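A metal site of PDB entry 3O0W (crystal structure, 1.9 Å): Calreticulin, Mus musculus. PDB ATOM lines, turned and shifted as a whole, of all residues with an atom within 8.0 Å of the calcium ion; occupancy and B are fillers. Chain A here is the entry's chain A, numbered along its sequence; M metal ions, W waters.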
ATOM      1  N   GLU A  11     -15.295 -22.378  -8.158  1.00  0.00           N
ATOM      2  CA  GLU A  11     -15.859 -21.177  -8.767  1.00  0.00           C
ATOM      3  C   GLU A  11     -15.662 -21.172 -10.281  1.00  0.00           C
ATOM      4  O   GLU A  11     -14.525 -21.100 -10.767  1.00  0.00           O
ATOM      5  CB  GLU A  11     -15.312 -19.891  -8.138  1.00  0.00           C
ATOM      6  CG  GLU A  11     -15.900 -18.624  -8.729  1.00  0.00           C
ATOM      7  CD  GLU A  11     -17.376 -18.439  -8.416  1.00  0.00           C
ATOM      8  OE1 GLU A  11     -17.683 -17.958  -7.307  1.00  0.00           O
ATOM      9  OE2 GLU A  11     -18.218 -18.765  -9.278  1.00  0.00           O
ATOM     10  N   GLN A  12     -16.774 -21.224 -10.992  1.00  0.00           N
ATOM     11  CA  GLN A  12     -16.770 -21.229 -12.434  1.00  0.00           C
ATOM     12  C   GLN A  12     -17.472 -20.016 -13.027  1.00  0.00           C
ATOM     13  O   GLN A  12     -17.397 -19.802 -14.234  1.00  0.00           O
ATOM     14  CB  GLN A  12     -17.403 -22.532 -12.941  1.00  0.00           C
ATOM     15  CG  GLN A  12     -16.521 -23.749 -12.725  1.00  0.00           C
ATOM     16  CD  GLN A  12     -17.152 -25.011 -13.243  1.00  0.00           C
ATOM     17  OE1 GLN A  12     -17.988 -25.618 -12.585  1.00  0.00           O
ATOM     18  NE2 GLN A  12     -16.761 -25.417 -14.447  1.00  0.00           N
ATOM     19  N   PHE A  13     -18.153 -19.224 -12.201  1.00  0.00           N
ATOM     20  CA  PHE A  13     -18.863 -18.021 -12.682  1.00  0.00           C
ATOM     21  C   PHE A  13     -19.878 -18.346 -13.779  1.00  0.00           C
ATOM     22  O   PHE A  13     -19.927 -17.685 -14.843  1.00  0.00           O
ATOM     23  CB  PHE A  13     -17.856 -16.980 -13.184  1.00  0.00           C
ATOM     24  CG  PHE A  13     -16.776 -16.638 -12.197  1.00  0.00           C
ATOM     25  CD1 PHE A  13     -17.039 -15.811 -11.110  1.00  0.00           C
ATOM     26  CD2 PHE A  13     -15.475 -17.121 -12.380  1.00  0.00           C
ATOM     27  CE1 PHE A  13     -16.046 -15.498 -10.202  1.00  0.00           C
ATOM     28  CE2 PHE A  13     -14.460 -16.811 -11.474  1.00  0.00           C
ATOM     29  CZ  PHE A  13     -14.751 -15.989 -10.387  1.00  0.00           C
ATOM     30  N   LEU A  14     -20.681 -19.372 -13.546  1.00  0.00           N
ATOM     31  CA  LEU A  14     -21.621 -19.844 -14.550  1.00  0.00           C
ATOM     32  C   LEU A  14     -23.007 -19.199 -14.435  1.00  0.00           C
ATOM     33  O   LEU A  14     -23.897 -19.445 -15.264  1.00  0.00           O
ATOM     34  CB  LEU A  14     -21.736 -21.363 -14.471  1.00  0.00           C
ATOM     35  CG  LEU A  14     -20.538 -22.178 -14.960  1.00  0.00           C
ATOM     36  CD1 LEU A  14     -20.642 -23.587 -14.438  1.00  0.00           C
ATOM     37  CD2 LEU A  14     -20.461 -22.183 -16.475  1.00  0.00           C
ATOM     38  N   ASP A  15     -23.197 -18.374 -13.411  1.00  0.00           N
ATOM     39  CA  ASP A  15     -24.538 -17.879 -13.101  1.00  0.00           C
ATOM     40  C   ASP A  15     -24.668 -16.361 -13.092  1.00  0.00           C
ATOM     41  O   ASP A  15     -25.291 -15.788 -12.191  1.00  0.00           O
ATOM     42  CB  ASP A  15     -25.032 -18.487 -11.765  1.00  0.00           C
ATOM     43  CG  ASP A  15     -24.043 -18.332 -10.631  1.00  0.00           C
ATOM     44  OD1 ASP A  15     -22.968 -17.720 -10.825  1.00  0.00           O
ATOM     45  OD2 ASP A  15     -24.370 -18.815  -9.523  1.00  0.00           O
ATOM     46  N   LEU A  37     -16.907  -9.276 -14.722  1.00  0.00           N
ATOM     47  CA  LEU A  37     -17.120 -10.615 -15.246  1.00  0.00           C
ATOM     48  C   LEU A  37     -17.176 -10.590 -16.782  1.00  0.00           C
ATOM     49  O   LEU A  37     -18.073  -9.964 -17.365  1.00  0.00           O
ATOM     50  CB  LEU A  37     -18.379 -11.250 -14.662  1.00  0.00           C
ATOM     51  CG  LEU A  37     -18.515 -12.770 -14.915  1.00  0.00           C
ATOM     52  CD1 LEU A  37     -17.744 -13.534 -13.870  1.00  0.00           C
ATOM     53  CD2 LEU A  37     -19.953 -13.205 -14.916  1.00  0.00           C
ATOM     54  N   SER A  38     -16.235 -11.283 -17.420  1.00  0.00           N
ATOM     55  CA  SER A  38     -16.111 -11.223 -18.877  1.00  0.00           C
ATOM     56  C   SER A  38     -15.490 -12.487 -19.498  1.00  0.00           C
ATOM     57  O   SER A  38     -14.640 -13.135 -18.889  1.00  0.00           O
ATOM     58  CB  SER A  38     -15.274 -10.015 -19.269  1.00  0.00           C
ATOM     59  OG  SER A  38     -15.205  -9.874 -20.672  1.00  0.00           O
ATOM     60  N   SER A  39     -15.923 -12.817 -20.720  1.00  0.00           N
ATOM     61  CA  SER A  39     -15.291 -13.877 -21.514  1.00  0.00           C
ATOM     62  C   SER A  39     -14.128 -13.331 -22.370  1.00  0.00           C
ATOM     63  O   SER A  39     -13.378 -14.090 -22.981  1.00  0.00           O
ATOM     64  CB  SER A  39     -16.316 -14.564 -22.429  1.00  0.00           C
ATOM     65  OG  SER A  39     -17.417 -15.122 -21.712  1.00  0.00           O
ATOM     66  N   ASP A  45     -15.870 -20.624 -25.401  1.00  0.00           N
ATOM     67  CA  ASP A  45     -17.323 -20.613 -25.333  1.00  0.00           C
ATOM     68  C   ASP A  45     -17.730 -19.375 -24.556  1.00  0.00           C
ATOM     69  O   ASP A  45     -17.199 -19.112 -23.468  1.00  0.00           O
ATOM     70  CB  ASP A  45     -17.838 -21.880 -24.631  1.00  0.00           C
ATOM     71  CG  ASP A  45     -19.344 -21.912 -24.491  1.00  0.00           C
ATOM     72  OD1 ASP A  45     -19.863 -21.381 -23.489  1.00  0.00           O
ATOM     73  OD2 ASP A  45     -20.009 -22.472 -25.377  1.00  0.00           O
ATOM     74  N   LEU A  46     -18.670 -18.608 -25.111  1.00  0.00           N
ATOM     75  CA  LEU A  46     -19.103 -17.361 -24.487  1.00  0.00           C
ATOM     76  C   LEU A  46     -19.541 -17.526 -23.032  1.00  0.00           C
ATOM     77  O   LEU A  46     -19.151 -16.731 -22.181  1.00  0.00           O
ATOM     78  CB  LEU A  46     -20.211 -16.676 -25.319  1.00  0.00           C
ATOM     79  CG  LEU A  46     -20.640 -15.291 -24.793  1.00  0.00           C
ATOM     80  CD1 LEU A  46     -19.547 -14.255 -24.987  1.00  0.00           C
ATOM     81  CD2 LEU A  46     -21.938 -14.803 -25.438  1.00  0.00           C
ATOM     82  N   GLU A  47     -20.346 -18.538 -22.744  1.00  0.00           N
ATOM     83  CA  GLU A  47     -20.903 -18.749 -21.404  1.00  0.00           C
ATOM     84  C   GLU A  47     -19.842 -19.327 -20.448  1.00  0.00           C
ATOM     85  O   GLU A  47     -19.653 -18.814 -19.349  1.00  0.00           O
ATOM     86  CB  GLU A  47     -22.137 -19.665 -21.455  1.00  0.00           C
ATOM     87  CG  GLU A  47     -23.306 -19.184 -22.362  1.00  0.00           C
ATOM     88  CD  GLU A  47     -24.337 -20.280 -22.673  1.00  0.00           C
ATOM     89  OE1 GLU A  47     -25.213 -20.530 -21.825  1.00  0.00           O
ATOM     90  OE2 GLU A  47     -24.283 -20.893 -23.762  1.00  0.00           O
ATOM     91  N   LYS A  48     -19.168 -20.386 -20.869  1.00  0.00           N
ATOM     92  CA  LYS A  48     -18.280 -21.146 -19.991  1.00  0.00           C
ATOM     93  C   LYS A  48     -17.045 -20.342 -19.607  1.00  0.00           C
ATOM     94  O   LYS A  48     -16.510 -20.510 -18.512  1.00  0.00           O
ATOM     95  CB  LYS A  48     -17.843 -22.462 -20.655  1.00  0.00           C
ATOM     96  CG  LYS A  48     -18.885 -23.583 -20.640  1.00  0.00           C
ATOM     97  CD  LYS A  48     -18.285 -24.782 -21.347  1.00  0.00           C
ATOM     98  CE  LYS A  48     -19.309 -25.807 -21.753  1.00  0.00           C
ATOM     99  NZ  LYS A  48     -18.599 -27.005 -22.295  1.00  0.00           N
ATOM    100  N   ASP A  49     -16.582 -19.487 -20.513  1.00  0.00           N
ATOM    101  CA  ASP A  49     -15.296 -18.816 -20.321  1.00  0.00           C
ATOM    102  C   ASP A  49     -15.394 -17.414 -19.703  1.00  0.00           C
ATOM    103  O   ASP A  49     -14.414 -16.668 -19.683  1.00  0.00           O
ATOM    104  CB  ASP A  49     -14.459 -18.878 -21.595  1.00  0.00           C
ATOM    105  CG  ASP A  49     -14.020 -20.307 -21.926  1.00  0.00           C
ATOM    106  OD1 ASP A  49     -13.531 -21.025 -21.010  1.00  0.00           O
ATOM    107  OD2 ASP A  49     -14.200 -20.724 -23.072  1.00  0.00           O
ATOM    108  N   LYS A  50     -16.571 -17.101 -19.184  1.00  0.00           N
ATOM    109  CA  LYS A  50     -16.744 -15.975 -18.276  1.00  0.00           C
ATOM    110  C   LYS A  50     -15.894 -16.213 -17.049  1.00  0.00           C
ATOM    111  O   LYS A  50     -15.933 -17.293 -16.449  1.00  0.00           O
ATOM    112  CB  LYS A  50     -18.194 -15.843 -17.834  1.00  0.00           C
ATOM    113  CG  LYS A  50     -19.162 -15.348 -18.896  1.00  0.00           C
ATOM    114  CD  LYS A  50     -19.132 -13.828 -19.024  1.00  0.00           C
ATOM    115  CE  LYS A  50     -20.328 -13.328 -19.823  1.00  0.00           C
ATOM    116  NZ  LYS A  50     -20.291 -13.822 -21.221  1.00  0.00           N
ATOM    117  N   GLY A  51     -15.148 -15.188 -16.660  1.00  0.00           N
ATOM    118  CA  GLY A  51     -14.395 -15.199 -15.421  1.00  0.00           C
ATOM    119  C   GLY A  51     -14.112 -13.784 -15.002  1.00  0.00           C
ATOM    120  O   GLY A  51     -14.575 -12.832 -15.649  1.00  0.00           O
ATOM    121  N   LEU A  52     -13.356 -13.642 -13.919  1.00  0.00           N
ATOM    122  CA  LEU A  52     -13.040 -12.328 -13.351  1.00  0.00           C
ATOM    123  C   LEU A  52     -11.910 -11.665 -14.113  1.00  0.00           C
ATOM    124  O   LEU A  52     -10.801 -12.181 -14.146  1.00  0.00           O
ATOM    125  CB  LEU A  52     -12.595 -12.468 -11.894  1.00  0.00           C
ATOM    126  CG  LEU A  52     -13.626 -12.821 -10.833  1.00  0.00           C
ATOM    127  CD1 LEU A  52     -12.917 -13.188  -9.535  1.00  0.00           C
ATOM    128  CD2 LEU A  52     -14.580 -11.664 -10.650  1.00  0.00           C
ATOM    129  N   THR A  82      -7.441 -21.241 -13.635  1.00  0.00           N
ATOM    130  CA  THR A  82      -6.919 -20.795 -14.932  1.00  0.00           C
ATOM    131  C   THR A  82      -6.646 -19.294 -14.914  1.00  0.00           C
ATOM    132  O   THR A  82      -7.341 -18.529 -14.240  1.00  0.00           O
ATOM    133  CB  THR A  82      -7.858 -21.145 -16.110  1.00  0.00           C
ATOM    134  OG1 THR A  82      -9.100 -20.470 -15.948  1.00  0.00           O
ATOM    135  CG2 THR A  82      -8.097 -22.670 -16.187  1.00  0.00           C
ATOM    136  N   ILE A 223      -7.900 -12.575 -17.128  1.00  0.00           N
ATOM    137  CA  ILE A 223      -9.136 -13.244 -16.729  1.00  0.00           C
ATOM    138  C   ILE A 223      -8.817 -14.508 -15.937  1.00  0.00           C
ATOM    139  O   ILE A 223      -8.024 -15.348 -16.363  1.00  0.00           O
ATOM    140  CB  ILE A 223     -10.047 -13.582 -17.935  1.00  0.00           C
ATOM    141  CG1 ILE A 223     -10.297 -12.338 -18.807  1.00  0.00           C
ATOM    142  CG2 ILE A 223     -11.355 -14.202 -17.460  1.00  0.00           C
ATOM    143  CD1 ILE A 223     -11.175 -12.601 -20.055  1.00  0.00           C
ATOM    144  N   PHE A 224      -9.440 -14.624 -14.766  1.00  0.00           N
ATOM    145  CA  PHE A 224      -9.268 -15.773 -13.878  1.00  0.00           C
ATOM    146  C   PHE A 224     -10.556 -16.617 -13.899  1.00  0.00           C
ATOM    147  O   PHE A 224     -11.650 -16.059 -13.875  1.00  0.00           O
ATOM    148  CB  PHE A 224      -9.010 -15.296 -12.448  1.00  0.00           C
ATOM    149  CG  PHE A 224      -7.753 -14.464 -12.295  1.00  0.00           C
ATOM    150  CD1 PHE A 224      -7.789 -13.077 -12.458  1.00  0.00           C
ATOM    151  CD2 PHE A 224      -6.536 -15.083 -11.996  1.00  0.00           C
ATOM    152  CE1 PHE A 224      -6.630 -12.309 -12.311  1.00  0.00           C
ATOM    153  CE2 PHE A 224      -5.375 -14.327 -11.862  1.00  0.00           C
ATOM    154  CZ  PHE A 224      -5.426 -12.931 -12.012  1.00  0.00           C
ATOM    155  N   ASP A 225     -10.433 -17.934 -13.915  1.00  0.00           N
ATOM    156  CA  ASP A 225     -11.629 -18.804 -14.006  1.00  0.00           C
ATOM    157  C   ASP A 225     -11.360 -20.153 -13.339  1.00  0.00           C
ATOM    158  O   ASP A 225     -10.215 -20.475 -12.979  1.00  0.00           O
ATOM    159  CB  ASP A 225     -11.991 -18.993 -15.492  1.00  0.00           C
ATOM    160  CG  ASP A 225     -13.451 -19.393 -15.711  1.00  0.00           C
ATOM    161  OD1 ASP A 225     -14.222 -19.546 -14.755  1.00  0.00           O
ATOM    162  OD2 ASP A 225     -13.840 -19.589 -16.887  1.00  0.00           O
ATOM    163  N   ASN A 226     -12.418 -20.934 -13.140  1.00  0.00           N
ATOM    164  CA  ASN A 226     -12.288 -22.354 -12.831  1.00  0.00           C
ATOM    165  C   ASN A 226     -11.439 -22.686 -11.588  1.00  0.00           C
ATOM    166  O   ASN A 226     -10.610 -23.594 -11.609  1.00  0.00           O
ATOM    167  CB  ASN A 226     -11.786 -23.079 -14.082  1.00  0.00           C
ATOM    168  CG  ASN A 226     -12.747 -22.920 -15.267  1.00  0.00           C
ATOM    169  OD1 ASN A 226     -12.373 -22.417 -16.339  1.00  0.00           O
ATOM    170  ND2 ASN A 226     -13.986 -23.328 -15.067  1.00  0.00           N
ATOM    171  N   PHE A 227     -11.666 -21.904 -10.534  1.00  0.00           N
ATOM    172  CA  PHE A 227     -11.018 -22.092  -9.249  1.00  0.00           C
ATOM    173  C   PHE A 227     -11.503 -23.399  -8.630  1.00  0.00           C
ATOM    174  O   PHE A 227     -12.689 -23.699  -8.661  1.00  0.00           O
ATOM    175  CB  PHE A 227     -11.366 -20.946  -8.291  1.00  0.00           C
ATOM    176  CG  PHE A 227     -10.775 -19.614  -8.676  1.00  0.00           C
ATOM    177  CD1 PHE A 227      -9.483 -19.263  -8.260  1.00  0.00           C
ATOM    178  CD2 PHE A 227     -11.510 -18.695  -9.431  1.00  0.00           C
ATOM    179  CE1 PHE A 227      -8.930 -18.024  -8.618  1.00  0.00           C
ATOM    180  CE2 PHE A 227     -10.970 -17.461  -9.779  1.00  0.00           C
ATOM    181  CZ  PHE A 227      -9.677 -17.121  -9.377  1.00  0.00           C
ATOM    182  N   THR A 243     -12.460 -28.481 -18.091  1.00  0.00           N
ATOM    183  CA  THR A 243     -12.545 -27.050 -17.930  1.00  0.00           C
ATOM    184  C   THR A 243     -11.550 -26.362 -18.880  1.00  0.00           C
ATOM    185  O   THR A 243     -11.921 -26.042 -20.009  1.00  0.00           O
ATOM    186  CB  THR A 243     -12.441 -26.714 -16.391  1.00  0.00           C
ATOM    187  OG1 THR A 243     -13.421 -25.753 -16.022  1.00  0.00           O
ATOM    188  CG2 THR A 243     -11.052 -26.354 -15.953  1.00  0.00           C
ATOM    189  N   THR A 247     -11.671 -25.447 -23.168  1.00  0.00           N
ATOM    190  CA  THR A 247     -11.489 -24.052 -23.571  1.00  0.00           C
ATOM    191  C   THR A 247     -10.430 -23.891 -24.674  1.00  0.00           C
ATOM    192  O   THR A 247     -10.638 -23.133 -25.636  1.00  0.00           O
ATOM    193  CB  THR A 247     -11.061 -23.175 -22.346  1.00  0.00           C
ATOM    194  OG1 THR A 247     -12.149 -23.104 -21.408  1.00  0.00           O
ATOM    195  CG2 THR A 247     -10.675 -21.747 -22.785  1.00  0.00           C
HETATM  196 CA    CA M   1     -16.273 -19.651 -16.294  1.00  0.00          CA
HETATM  197  O   HOH W   1     -16.139 -22.069 -16.235  1.00  0.00           O
HETATM  198  O   HOH W   2     -18.499 -19.128 -16.893  1.00  0.00           O
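Water W2 lies within hydrogen-bond range of the backbone carbonyl oxygen (O) of Glu 47 (2.7 Å) and the backbone carbonyl oxygen (O) of Phe 13 (2.9 Å).
Four residues have an atom within 4 Å of the calcium ion: Gln 12, Lys 48, Lys 50 and Asp 225. The nearest printed residue that does not touch the calcium ion is Asp 49 (4.2 Å).
The side-chain amino group (NZ) of Lys 50 sits at hydrogen-bond distance from the side-chain hydroxyl (OG) of Ser 39 (3.2 Å). The backbone carbonyl oxygen of Leu 46 lies within hydrogen-bond range of the side-chain amino group of Lys 50, 3.3 Å away. OD1 of Asp 45 is in hydrogen-bond range of N of Lys 48 (2.9 Å). The side-chain carboxylate (OD2) of Asp 225 sits close to the side-chain amide oxygen (OD1) of Asn 226, at 3.2 Å. The backbone NH (N) of Thr 82 lies within hydrogen-bond range of the backbone carbonyl oxygen (O) of Asp 225, at 3.0 Å.
The calcium ion is bound by O of Gln 12 (2.4 Å), water W2 (2.4 Å), O of Lys 50 (2.4 Å), O of Lys 48 (2.4 Å), water W1 (2.4 Å), OD2 of Asp 225 (2.5 Å) and OD1 of Asp 225 (2.6 Å). The calcium ion has seven donor atoms within binding distance.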
